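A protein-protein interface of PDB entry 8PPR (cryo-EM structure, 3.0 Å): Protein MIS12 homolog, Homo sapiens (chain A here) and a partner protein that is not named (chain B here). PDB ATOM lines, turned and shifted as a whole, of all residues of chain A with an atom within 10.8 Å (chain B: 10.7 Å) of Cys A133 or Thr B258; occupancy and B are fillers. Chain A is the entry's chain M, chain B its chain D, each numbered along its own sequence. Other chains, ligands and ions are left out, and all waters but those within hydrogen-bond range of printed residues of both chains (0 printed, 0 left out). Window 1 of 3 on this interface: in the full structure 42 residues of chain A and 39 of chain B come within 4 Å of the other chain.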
ATOM      1  N   GLN A 123      34.226  29.126 -22.538  1.00  0.00           N
ATOM      2  CA  GLN A 123      33.030  28.565 -21.923  1.00  0.00           C
ATOM      3  C   GLN A 123      31.790  28.866 -22.754  1.00  0.00           C
ATOM      4  O   GLN A 123      30.921  28.004 -22.923  1.00  0.00           O
ATOM      5  CB  GLN A 123      32.872  29.108 -20.505  1.00  0.00           C
ATOM      6  CG  GLN A 123      33.878  28.537 -19.524  1.00  0.00           C
ATOM      7  CD  GLN A 123      33.885  27.024 -19.520  1.00  0.00           C
ATOM      8  OE1 GLN A 123      32.877  26.387 -19.217  1.00  0.00           O
ATOM      9  NE2 GLN A 123      35.027  26.438 -19.864  1.00  0.00           N
ATOM     10  N   GLN A 125      31.779  29.385 -25.970  1.00  0.00           N
ATOM     11  CA  GLN A 125      31.891  28.539 -27.152  1.00  0.00           C
ATOM     12  C   GLN A 125      31.366  27.139 -26.870  1.00  0.00           C
ATOM     13  O   GLN A 125      30.656  26.554 -27.696  1.00  0.00           O
ATOM     14  CB  GLN A 125      33.347  28.478 -27.614  1.00  0.00           C
ATOM     15  CG  GLN A 125      33.762  29.616 -28.529  1.00  0.00           C
ATOM     16  CD  GLN A 125      34.946  29.260 -29.403  1.00  0.00           C
ATOM     17  OE1 GLN A 125      35.583  28.224 -29.211  1.00  0.00           O
ATOM     18  NE2 GLN A 125      35.248  30.116 -30.370  1.00  0.00           N
ATOM     19  N   GLU A 126      31.706  26.588 -25.705  1.00  0.00           N
ATOM     20  CA  GLU A 126      31.173  25.281 -25.325  1.00  0.00           C
ATOM     21  C   GLU A 126      29.657  25.328 -25.167  1.00  0.00           C
ATOM     22  O   GLU A 126      28.942  24.422 -25.621  1.00  0.00           O
ATOM     23  CB  GLU A 126      31.828  24.810 -24.027  1.00  0.00           C
ATOM     24  CG  GLU A 126      33.271  24.383 -24.190  1.00  0.00           C
ATOM     25  CD  GLU A 126      33.461  23.427 -25.347  1.00  0.00           C
ATOM     26  OE1 GLU A 126      32.805  22.365 -25.353  1.00  0.00           O
ATOM     27  OE2 GLU A 126      34.263  23.739 -26.252  1.00  0.00           O
ATOM     28  N   LYS A 127      29.153  26.383 -24.527  1.00  0.00           N
ATOM     29  CA  LYS A 127      27.728  26.489 -24.243  1.00  0.00           C
ATOM     30  C   LYS A 127      26.902  26.599 -25.515  1.00  0.00           C
ATOM     31  O   LYS A 127      25.783  26.080 -25.569  1.00  0.00           O
ATOM     32  CB  LYS A 127      27.469  27.693 -23.341  1.00  0.00           C
ATOM     33  CG  LYS A 127      27.566  27.386 -21.860  1.00  0.00           C
ATOM     34  CD  LYS A 127      27.794  28.654 -21.058  1.00  0.00           C
ATOM     35  CE  LYS A 127      26.666  29.650 -21.273  1.00  0.00           C
ATOM     36  NZ  LYS A 127      25.329  29.008 -21.153  1.00  0.00           N
ATOM     37  N   TYR A 128      27.422  27.283 -26.534  1.00  0.00           N
ATOM     38  CA  TYR A 128      26.694  27.398 -27.794  1.00  0.00           C
ATOM     39  C   TYR A 128      26.447  26.025 -28.409  1.00  0.00           C
ATOM     40  O   TYR A 128      25.322  25.700 -28.816  1.00  0.00           O
ATOM     41  CB  TYR A 128      27.474  28.291 -28.757  1.00  0.00           C
ATOM     42  CG  TYR A 128      26.703  28.692 -29.990  1.00  0.00           C
ATOM     43  CD1 TYR A 128      25.614  29.549 -29.903  1.00  0.00           C
ATOM     44  CD2 TYR A 128      27.066  28.216 -31.243  1.00  0.00           C
ATOM     45  CE1 TYR A 128      24.908  29.920 -31.029  1.00  0.00           C
ATOM     46  CE2 TYR A 128      26.366  28.583 -32.375  1.00  0.00           C
ATOM     47  CZ  TYR A 128      25.288  29.434 -32.262  1.00  0.00           C
ATOM     48  OH  TYR A 128      24.588  29.800 -33.389  1.00  0.00           O
ATOM     49  N   LYS A 129      27.492  25.199 -28.470  1.00  0.00           N
ATOM     50  CA  LYS A 129      27.347  23.848 -28.999  1.00  0.00           C
ATOM     51  C   LYS A 129      26.418  23.016 -28.128  1.00  0.00           C
ATOM     52  O   LYS A 129      25.615  22.221 -28.638  1.00  0.00           O
ATOM     53  CB  LYS A 129      28.719  23.187 -29.105  1.00  0.00           C
ATOM     54  CG  LYS A 129      29.583  23.731 -30.226  1.00  0.00           C
ATOM     55  CD  LYS A 129      31.010  23.949 -29.751  1.00  0.00           C
ATOM     56  CE  LYS A 129      31.617  22.664 -29.218  1.00  0.00           C
ATOM     57  NZ  LYS A 129      33.104  22.733 -29.173  1.00  0.00           N
ATOM     58  N   THR A 130      26.520  23.180 -26.806  1.00  0.00           N
ATOM     59  CA  THR A 130      25.631  22.453 -25.906  1.00  0.00           C
ATOM     60  C   THR A 130      24.171  22.788 -26.183  1.00  0.00           C
ATOM     61  O   THR A 130      23.321  21.892 -26.259  1.00  0.00           O
ATOM     62  CB  THR A 130      25.990  22.771 -24.455  1.00  0.00           C
ATOM     63  OG1 THR A 130      27.286  22.240 -24.153  1.00  0.00           O
ATOM     64  CG2 THR A 130      24.968  22.173 -23.511  1.00  0.00           C
ATOM     65  N   GLU A 131      23.864  24.074 -26.354  1.00  0.00           N
ATOM     66  CA  GLU A 131      22.491  24.482 -26.632  1.00  0.00           C
ATOM     67  C   GLU A 131      22.024  23.989 -27.995  1.00  0.00           C
ATOM     68  O   GLU A 131      20.858  23.613 -28.157  1.00  0.00           O
ATOM     69  CB  GLU A 131      22.361  26.002 -26.535  1.00  0.00           C
ATOM     70  CG  GLU A 131      22.712  26.571 -25.176  1.00  0.00           C
ATOM     71  CD  GLU A 131      21.665  26.257 -24.126  1.00  0.00           C
ATOM     72  OE1 GLU A 131      20.557  25.814 -24.497  1.00  0.00           O
ATOM     73  OE2 GLU A 131      21.949  26.451 -22.926  1.00  0.00           O
ATOM     74  N   LEU A 132      22.912  23.997 -28.994  1.00  0.00           N
ATOM     75  CA  LEU A 132      22.536  23.461 -30.300  1.00  0.00           C
ATOM     76  C   LEU A 132      22.170  21.984 -30.203  1.00  0.00           C
ATOM     77  O   LEU A 132      21.148  21.543 -30.753  1.00  0.00           O
ATOM     78  CB  LEU A 132      23.677  23.665 -31.295  1.00  0.00           C
ATOM     79  CG  LEU A 132      23.817  25.071 -31.878  1.00  0.00           C
ATOM     80  CD1 LEU A 132      25.109  25.197 -32.670  1.00  0.00           C
ATOM     81  CD2 LEU A 132      22.617  25.407 -32.746  1.00  0.00           C
ATOM     82  N   CYS A 133      22.988  21.210 -29.488  1.00  0.00           N
ATOM     83  CA  CYS A 133      22.695  19.793 -29.306  1.00  0.00           C
ATOM     84  C   CYS A 133      21.388  19.598 -28.549  1.00  0.00           C
ATOM     85  O   CYS A 133      20.597  18.701 -28.872  1.00  0.00           O
ATOM     86  CB  CYS A 133      23.850  19.118 -28.570  1.00  0.00           C
ATOM     87  SG  CYS A 133      25.389  19.057 -29.516  1.00  0.00           S
ATOM     88  N   THR A 134      21.152  20.425 -27.529  1.00  0.00           N
ATOM     89  CA  THR A 134      19.908  20.339 -26.773  1.00  0.00           C
ATOM     90  C   THR A 134      18.705  20.602 -27.665  1.00  0.00           C
ATOM     91  O   THR A 134      17.691  19.901 -27.578  1.00  0.00           O
ATOM     92  CB  THR A 134      19.936  21.332 -25.614  1.00  0.00           C
ATOM     93  OG1 THR A 134      21.060  21.049 -24.773  1.00  0.00           O
ATOM     94  CG2 THR A 134      18.656  21.236 -24.799  1.00  0.00           C
ATOM     95  N   LYS A 135      18.800  21.613 -28.529  1.00  0.00           N
ATOM     96  CA  LYS A 135      17.710  21.902 -29.453  1.00  0.00           C
ATOM     97  C   LYS A 135      17.457  20.725 -30.386  1.00  0.00           C
ATOM     98  O   LYS A 135      16.302  20.365 -30.648  1.00  0.00           O
ATOM     99  CB  LYS A 135      18.026  23.166 -30.250  1.00  0.00           C
ATOM    100  CG  LYS A 135      17.399  23.206 -31.630  1.00  0.00           C
ATOM    101  CD  LYS A 135      17.812  24.456 -32.384  1.00  0.00           C
ATOM    102  CE  LYS A 135      17.347  24.406 -33.829  1.00  0.00           C
ATOM    103  NZ  LYS A 135      17.613  25.685 -34.541  1.00  0.00           N
ATOM    104  N   GLN A 136      18.527  20.109 -30.895  1.00  0.00           N
ATOM    105  CA  GLN A 136      18.352  18.950 -31.767  1.00  0.00           C
ATOM    106  C   GLN A 136      17.647  17.811 -31.036  1.00  0.00           C
ATOM    107  O   GLN A 136      16.723  17.182 -31.576  1.00  0.00           O
ATOM    108  CB  GLN A 136      19.709  18.488 -32.296  1.00  0.00           C
ATOM    109  CG  GLN A 136      20.267  19.360 -33.404  1.00  0.00           C
ATOM    110  CD  GLN A 136      19.222  19.725 -34.437  1.00  0.00           C
ATOM    111  OE1 GLN A 136      18.594  18.853 -35.038  1.00  0.00           O
ATOM    112  NE2 GLN A 136      19.027  21.022 -34.647  1.00  0.00           N
ATOM    113  N   ALA A 137      18.060  17.545 -29.795  1.00  0.00           N
ATOM    114  CA  ALA A 137      17.422  16.492 -29.014  1.00  0.00           C
ATOM    115  C   ALA A 137      15.955  16.810 -28.759  1.00  0.00           C
ATOM    116  O   ALA A 137      15.102  15.915 -28.777  1.00  0.00           O
ATOM    117  CB  ALA A 137      18.167  16.291 -27.695  1.00  0.00           C
ATOM    118  N   LEU A 138      15.642  18.084 -28.519  1.00  0.00           N
ATOM    119  CA  LEU A 138      14.255  18.470 -28.288  1.00  0.00           C
ATOM    120  C   LEU A 138      13.410  18.280 -29.542  1.00  0.00           C
ATOM    121  O   LEU A 138      12.257  17.846 -29.456  1.00  0.00           O
ATOM    122  CB  LEU A 138      14.190  19.912 -27.790  1.00  0.00           C
ATOM    123  CG  LEU A 138      14.783  20.096 -26.389  1.00  0.00           C
ATOM    124  CD1 LEU A 138      14.381  21.423 -25.776  1.00  0.00           C
ATOM    125  CD2 LEU A 138      14.373  18.946 -25.481  1.00  0.00           C
ATOM    126  N   LEU A 139      13.962  18.598 -30.715  1.00  0.00           N
ATOM    127  CA  LEU A 139      13.239  18.318 -31.955  1.00  0.00           C
ATOM    128  C   LEU A 139      12.975  16.826 -32.114  1.00  0.00           C
ATOM    129  O   LEU A 139      11.874  16.415 -32.514  1.00  0.00           O
ATOM    130  CB  LEU A 139      14.012  18.854 -33.160  1.00  0.00           C
ATOM    131  CG  LEU A 139      13.692  20.271 -33.642  1.00  0.00           C
ATOM    132  CD1 LEU A 139      14.198  21.328 -32.683  1.00  0.00           C
ATOM    133  CD2 LEU A 139      14.267  20.493 -35.033  1.00  0.00           C
ATOM    134  N   ALA A 140      13.975  15.997 -31.805  1.00  0.00           N
ATOM    135  CA  ALA A 140      13.766  14.552 -31.865  1.00  0.00           C
ATOM    136  C   ALA A 140      12.656  14.117 -30.914  1.00  0.00           C
ATOM    137  O   ALA A 140      11.817  13.273 -31.260  1.00  0.00           O
ATOM    138  CB  ALA A 140      15.068  13.819 -31.545  1.00  0.00           C
ATOM    139  N   GLU A 141      12.637  14.689 -29.707  1.00  0.00           N
ATOM    140  CA  GLU A 141      11.599  14.346 -28.742  1.00  0.00           C
ATOM    141  C   GLU A 141      10.220  14.765 -29.236  1.00  0.00           C
ATOM    142  O   GLU A 141       9.242  14.039 -29.040  1.00  0.00           O
ATOM    143  CB  GLU A 141      11.897  14.989 -27.388  1.00  0.00           C
ATOM    144  CG  GLU A 141      11.002  14.476 -26.273  1.00  0.00           C
ATOM    145  CD  GLU A 141      11.569  14.741 -24.895  1.00  0.00           C
ATOM    146  OE1 GLU A 141      12.714  15.233 -24.807  1.00  0.00           O
ATOM    147  OE2 GLU A 141      10.872  14.455 -23.898  1.00  0.00           O
ATOM    148  N   THR B 250      30.347  16.692 -42.034  1.00  0.00           N
ATOM    149  CA  THR B 250      30.865  15.896 -40.924  1.00  0.00           C
ATOM    150  C   THR B 250      29.809  15.883 -39.822  1.00  0.00           C
ATOM    151  O   THR B 250      29.830  16.699 -38.899  1.00  0.00           O
ATOM    152  CB  THR B 250      32.203  16.455 -40.422  1.00  0.00           C
ATOM    153  OG1 THR B 250      33.073  16.693 -41.537  1.00  0.00           O
ATOM    154  CG2 THR B 250      32.868  15.471 -39.470  1.00  0.00           C
ATOM    155  N   GLU B 251      28.876  14.941 -39.927  1.00  0.00           N
ATOM    156  CA  GLU B 251      27.851  14.792 -38.903  1.00  0.00           C
ATOM    157  C   GLU B 251      28.448  14.141 -37.663  1.00  0.00           C
ATOM    158  O   GLU B 251      29.126  13.113 -37.753  1.00  0.00           O
ATOM    159  CB  GLU B 251      26.687  13.959 -39.436  1.00  0.00           C
ATOM    160  CG  GLU B 251      25.788  14.705 -40.406  1.00  0.00           C
ATOM    161  CD  GLU B 251      24.699  13.824 -40.984  1.00  0.00           C
ATOM    162  OE1 GLU B 251      24.664  12.622 -40.645  1.00  0.00           O
ATOM    163  OE2 GLU B 251      23.880  14.333 -41.776  1.00  0.00           O
ATOM    164  N   VAL B 252      28.198  14.741 -36.503  1.00  0.00           N
ATOM    165  CA  VAL B 252      28.752  14.278 -35.238  1.00  0.00           C
ATOM    166  C   VAL B 252      27.605  13.881 -34.322  1.00  0.00           C
ATOM    167  O   VAL B 252      26.707  14.690 -34.057  1.00  0.00           O
ATOM    168  CB  VAL B 252      29.631  15.353 -34.573  1.00  0.00           C
ATOM    169  CG1 VAL B 252      30.360  14.773 -33.372  1.00  0.00           C
ATOM    170  CG2 VAL B 252      30.617  15.929 -35.578  1.00  0.00           C
ATOM    171  N   LYS B 253      27.636  12.641 -33.844  1.00  0.00           N
ATOM    172  CA  LYS B 253      26.670  12.202 -32.850  1.00  0.00           C
ATOM    173  C   LYS B 253      26.961  12.852 -31.503  1.00  0.00           C
ATOM    174  O   LYS B 253      28.111  13.143 -31.162  1.00  0.00           O
ATOM    175  CB  LYS B 253      26.685  10.678 -32.721  1.00  0.00           C
ATOM    176  CG  LYS B 253      25.947   9.929 -33.832  1.00  0.00           C
ATOM    177  CD  LYS B 253      24.707  10.672 -34.330  1.00  0.00           C
ATOM    178  CE  LYS B 253      23.622  10.750 -33.253  1.00  0.00           C
ATOM    179  NZ  LYS B 253      22.319  11.215 -33.792  1.00  0.00           N
ATOM    180  N   VAL B 254      25.901  13.078 -30.735  1.00  0.00           N
ATOM    181  CA  VAL B 254      25.980  13.807 -29.475  1.00  0.00           C
ATOM    182  C   VAL B 254      25.886  12.808 -28.331  1.00  0.00           C
ATOM    183  O   VAL B 254      24.908  12.055 -28.229  1.00  0.00           O
ATOM    184  CB  VAL B 254      24.878  14.869 -29.366  1.00  0.00           C
ATOM    185  CG1 VAL B 254      25.130  15.757 -28.164  1.00  0.00           C
ATOM    186  CG2 VAL B 254      24.807  15.690 -30.645  1.00  0.00           C
ATOM    187  N   GLU B 255      26.899  12.805 -27.478  1.00  0.00           N
ATOM    188  CA  GLU B 255      26.914  11.996 -26.274  1.00  0.00           C
ATOM    189  C   GLU B 255      26.140  12.693 -25.154  1.00  0.00           C
ATOM    190  O   GLU B 255      26.006  13.920 -25.155  1.00  0.00           O
ATOM    191  CB  GLU B 255      28.351  11.732 -25.840  1.00  0.00           C
ATOM    192  CG  GLU B 255      29.171  12.989 -25.626  1.00  0.00           C
ATOM    193  CD  GLU B 255      29.893  13.434 -26.884  1.00  0.00           C
ATOM    194  OE1 GLU B 255      29.548  12.939 -27.977  1.00  0.00           O
ATOM    195  OE2 GLU B 255      30.807  14.278 -26.778  1.00  0.00           O
ATOM    196  N   PRO B 256      25.607  11.929 -24.196  1.00  0.00           N
ATOM    197  CA  PRO B 256      24.775  12.546 -23.147  1.00  0.00           C
ATOM    198  C   PRO B 256      25.497  13.591 -22.316  1.00  0.00           C
ATOM    199  O   PRO B 256      24.853  14.535 -21.841  1.00  0.00           O
ATOM    200  CB  PRO B 256      24.346  11.345 -22.290  1.00  0.00           C
ATOM    201  CG  PRO B 256      24.486  10.162 -23.184  1.00  0.00           C
ATOM    202  CD  PRO B 256      25.645  10.461 -24.080  1.00  0.00           C
ATOM    203  N   MET B 257      26.812  13.455 -22.119  1.00  0.00           N
ATOM    204  CA  MET B 257      27.532  14.420 -21.291  1.00  0.00           C
ATOM    205  C   MET B 257      27.517  15.814 -21.905  1.00  0.00           C
ATOM    206  O   MET B 257      27.718  16.806 -21.195  1.00  0.00           O
ATOM    207  CB  MET B 257      28.968  13.945 -21.048  1.00  0.00           C
ATOM    208  CG  MET B 257      29.828  13.776 -22.295  1.00  0.00           C
ATOM    209  SD  MET B 257      30.513  15.302 -22.977  1.00  0.00           S
ATOM    210  CE  MET B 257      31.729  15.715 -21.730  1.00  0.00           C
ATOM    211  N   THR B 258      27.292  15.912 -23.218  1.00  0.00           N
ATOM    212  CA  THR B 258      27.153  17.221 -23.845  1.00  0.00           C
ATOM    213  C   THR B 258      25.958  17.979 -23.285  1.00  0.00           C
ATOM    214  O   THR B 258      26.007  19.206 -23.146  1.00  0.00           O
ATOM    215  CB  THR B 258      27.022  17.066 -25.361  1.00  0.00           C
ATOM    216  OG1 THR B 258      28.119  16.291 -25.860  1.00  0.00           O
ATOM    217  CG2 THR B 258      27.022  18.427 -26.043  1.00  0.00           C
ATOM    218  N   TYR B 259      24.887  17.267 -22.943  1.00  0.00           N
ATOM    219  CA  TYR B 259      23.683  17.872 -22.391  1.00  0.00           C
ATOM    220  C   TYR B 259      23.781  18.138 -20.896  1.00  0.00           C
ATOM    221  O   TYR B 259      22.845  18.703 -20.321  1.00  0.00           O
ATOM    222  CB  TYR B 259      22.474  16.973 -22.665  1.00  0.00           C
ATOM    223  CG  TYR B 259      22.308  16.592 -24.117  1.00  0.00           C
ATOM    224  CD1 TYR B 259      21.953  17.540 -25.066  1.00  0.00           C
ATOM    225  CD2 TYR B 259      22.505  15.284 -24.539  1.00  0.00           C
ATOM    226  CE1 TYR B 259      21.798  17.196 -26.391  1.00  0.00           C
ATOM    227  CE2 TYR B 259      22.352  14.931 -25.865  1.00  0.00           C
ATOM    228  CZ  TYR B 259      21.997  15.893 -26.787  1.00  0.00           C
ATOM    229  OH  TYR B 259      21.844  15.551 -28.111  1.00  0.00           O
ATOM    230  N   LEU B 260      24.883  17.739 -20.253  1.00  0.00           N
ATOM    231  CA  LEU B 260      25.005  17.922 -18.811  1.00  0.00           C
ATOM    232  C   LEU B 260      25.013  19.394 -18.425  1.00  0.00           C
ATOM    233  O   LEU B 260      24.386  19.776 -17.431  1.00  0.00           O
ATOM    234  CB  LEU B 260      26.272  17.234 -18.303  1.00  0.00           C
ATOM    235  CG  LEU B 260      26.184  15.716 -18.142  1.00  0.00           C
ATOM    236  CD1 LEU B 260      27.309  15.204 -17.256  1.00  0.00           C
ATOM    237  CD2 LEU B 260      24.827  15.304 -17.587  1.00  0.00           C
ATOM    238  N   GLY B 261      25.705  20.231 -19.191  1.00  0.00           N
ATOM    239  CA  GLY B 261      25.737  21.653 -18.945  1.00  0.00           C
ATOM    240  C   GLY B 261      24.612  22.428 -19.591  1.00  0.00           C
ATOM    241  O   GLY B 261      24.621  23.663 -19.551  1.00  0.00           O
ATOM    242  N   SER B 262      23.644  21.741 -20.188  1.00  0.00           N
ATOM    243  CA  SER B 262      22.555  22.412 -20.874  1.00  0.00           C
ATOM    244  C   SER B 262      21.607  23.074 -19.879  1.00  0.00           C
ATOM    245  O   SER B 262      21.440  22.627 -18.740  1.00  0.00           O
ATOM    246  CB  SER B 262      21.782  21.425 -21.745  1.00  0.00           C
ATOM    247  OG  SER B 262      20.936  22.109 -22.650  1.00  0.00           O
ATOM    248  N   SER B 263      20.983  24.163 -20.331  1.00  0.00           N
ATOM    249  CA  SER B 263      19.992  24.844 -19.505  1.00  0.00           C
ATOM    250  C   SER B 263      18.783  23.953 -19.248  1.00  0.00           C
ATOM    251  O   SER B 263      18.286  23.882 -18.119  1.00  0.00           O
ATOM    252  CB  SER B 263      19.564  26.151 -20.171  1.00  0.00           C
ATOM    253  OG  SER B 263      18.902  25.902 -21.398  1.00  0.00           O
ATOM    254  N   GLN B 264      18.300  23.267 -20.279  1.00  0.00           N
ATOM    255  CA  GLN B 264      17.156  22.367 -20.140  1.00  0.00           C
ATOM    256  C   GLN B 264      17.607  20.941 -19.844  1.00  0.00           C
ATOM    257  O   GLN B 264      17.197  19.983 -20.497  1.00  0.00           O
ATOM    258  CB  GLN B 264      16.301  22.421 -21.400  1.00  0.00           C
ATOM    259  CG  GLN B 264      15.941  23.831 -21.842  1.00  0.00           C
ATOM    260  CD  GLN B 264      14.854  24.460 -20.992  1.00  0.00           C
ATOM    261  OE1 GLN B 264      14.442  23.908 -19.972  1.00  0.00           O
ATOM    262  NE2 GLN B 264      14.384  25.628 -21.411  1.00  0.00           N
ATOM    263  N   ASN B 265      18.469  20.800 -18.836  1.00  0.00           N
ATOM    264  CA  ASN B 265      18.967  19.479 -18.472  1.00  0.00           C
ATOM    265  C   ASN B 265      17.869  18.627 -17.853  1.00  0.00           C
ATOM    266  O   ASN B 265      17.791  17.420 -18.112  1.00  0.00           O
ATOM    267  CB  ASN B 265      20.152  19.613 -17.518  1.00  0.00           C
ATOM    268  CG  ASN B 265      20.938  18.327 -17.387  1.00  0.00           C
ATOM    269  OD1 ASN B 265      20.930  17.487 -18.286  1.00  0.00           O
ATOM    270  ND2 ASN B 265      21.626  18.166 -16.263  1.00  0.00           N
ATOM    271  N   LEU B 268      15.477  17.170 -20.557  1.00  0.00           N
ATOM    272  CA  LEU B 268      16.119  16.072 -21.269  1.00  0.00           C
ATOM    273  C   LEU B 268      16.214  14.829 -20.395  1.00  0.00           C
ATOM    274  O   LEU B 268      15.983  13.710 -20.867  1.00  0.00           O
ATOM    275  CB  LEU B 268      17.510  16.498 -21.737  1.00  0.00           C
ATOM    276  CG  LEU B 268      17.573  17.544 -22.850  1.00  0.00           C
ATOM    277  CD1 LEU B 268      18.960  18.162 -22.907  1.00  0.00           C
ATOM    278  CD2 LEU B 268      17.199  16.929 -24.187  1.00  0.00           C
ATOM    279  N   ASN B 269      16.552  15.008 -19.118  1.00  0.00           N
ATOM    280  CA  ASN B 269      16.756  13.867 -18.235  1.00  0.00           C
ATOM    281  C   ASN B 269      15.446  13.150 -17.937  1.00  0.00           C
ATOM    282  O   ASN B 269      15.422  11.923 -17.793  1.00  0.00           O
ATOM    283  CB  ASN B 269      17.422  14.330 -16.941  1.00  0.00           C
ATOM    284  CG  ASN B 269      18.932  14.265 -17.011  1.00  0.00           C
ATOM    285  OD1 ASN B 269      19.496  13.579 -17.862  1.00  0.00           O
ATOM    286  ND2 ASN B 269      19.598  14.988 -16.118  1.00  0.00           N
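O of Thr B258 sits close to OG1 of Thr A130 (3.4 Å). The side-chain hydroxyl of Tyr B259 sits close to the backbone carbonyl oxygen of Cys A133 (3.5 Å). OG of Ser B263 lies within hydrogen-bond range of OE2 of Glu A131 (3.5 Å). The side-chain hydroxyl (OG1) of Thr A134 sits close to the side-chain hydroxyl (OG) of Ser B262.
OG1 of Thr B258 sits at hydrogen-bond distance from O of Glu B255 (3.3 Å). The backbone carbonyl oxygen (O) of Tyr B259 sits close to the side-chain amide oxygen (OD1) of Asn B265. The backbone carbonyl oxygen (O) of Glu A126 is in hydrogen-bond range of the side-chain hydroxyl (OG1) of Thr A130, at 3.1 Å. The side-chain sulfur (SG) of Cys A133 is in hydrogen-bond range of the backbone carbonyl oxygen (O) of Lys A129 (3.3 Å). O of Thr A130 is in hydrogen-bond range of OG1 of Thr A134, at 2.8 Å.
Gly B261 touches Thr A130 (C to CG2, 3.9 Å). CA of Ser B262 touches CG2 of Thr A130 (3.6 Å). Cys A133 touches Val B254. Cys A133 touches Thr B258. N of Thr A134 touches CE1 of Tyr B259 (3.5 Å). CG2 of Thr A134 touches CD1 of Leu B268, at 3.6 Å. Ala A137 touches Tyr B259 (CB to OH, 3.8 Å). Leu B268 touches Ala A137. Leu A138 touches Leu B268.
Gln A123 touches none of the printed residues of chain B. Printed residues of chain B within 4 Å of Glu A131: Ser B263 (3.5 Å). Of chain B, only Val B254, Thr B258 and Tyr B259 come within 4 Å of Cys A133. Thr A134 touches three residues of chain B. No residue of chain B comes within 4 Å of Gln A136. Of the printed residues of chain B, Leu A138 touches Leu B268. Lys B253 touches none of the printed residues of chain A. No residue of chain A comes within 4 Å of Glu B255. No residue of chain A comes within 4 Å of Pro B256. Thr B258 touches two residues of chain A. Tyr B259 touches just these residues of chain A: Cys A133, Thr A134 and Ala A137. No residue of chain A comes within 4 Å of Leu B260. Gly B261 touches one residue of chain A. Of the printed residues of chain A, Ser B262 touches Thr A130 (3.6 Å) and Thr A134 (2.4 Å). Printed residues of chain A within 4 Å of Ser B263: Glu A131 (3.5 Å). Of the printed residues of chain A, Leu B268 touches Thr A134, Ala A137 and Leu A138. The nearest printed residue of chain A that does not touch Ser B262 is Glu A131 (4.2 Å).
Hydrophobic or aromatic side chains of chain B within 4 Å of the printed part of chain A: Val B254, Tyr B259 and Leu B268. Along chain B the printed residues that touch a printed residue of chain A span positions 254 to 268.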
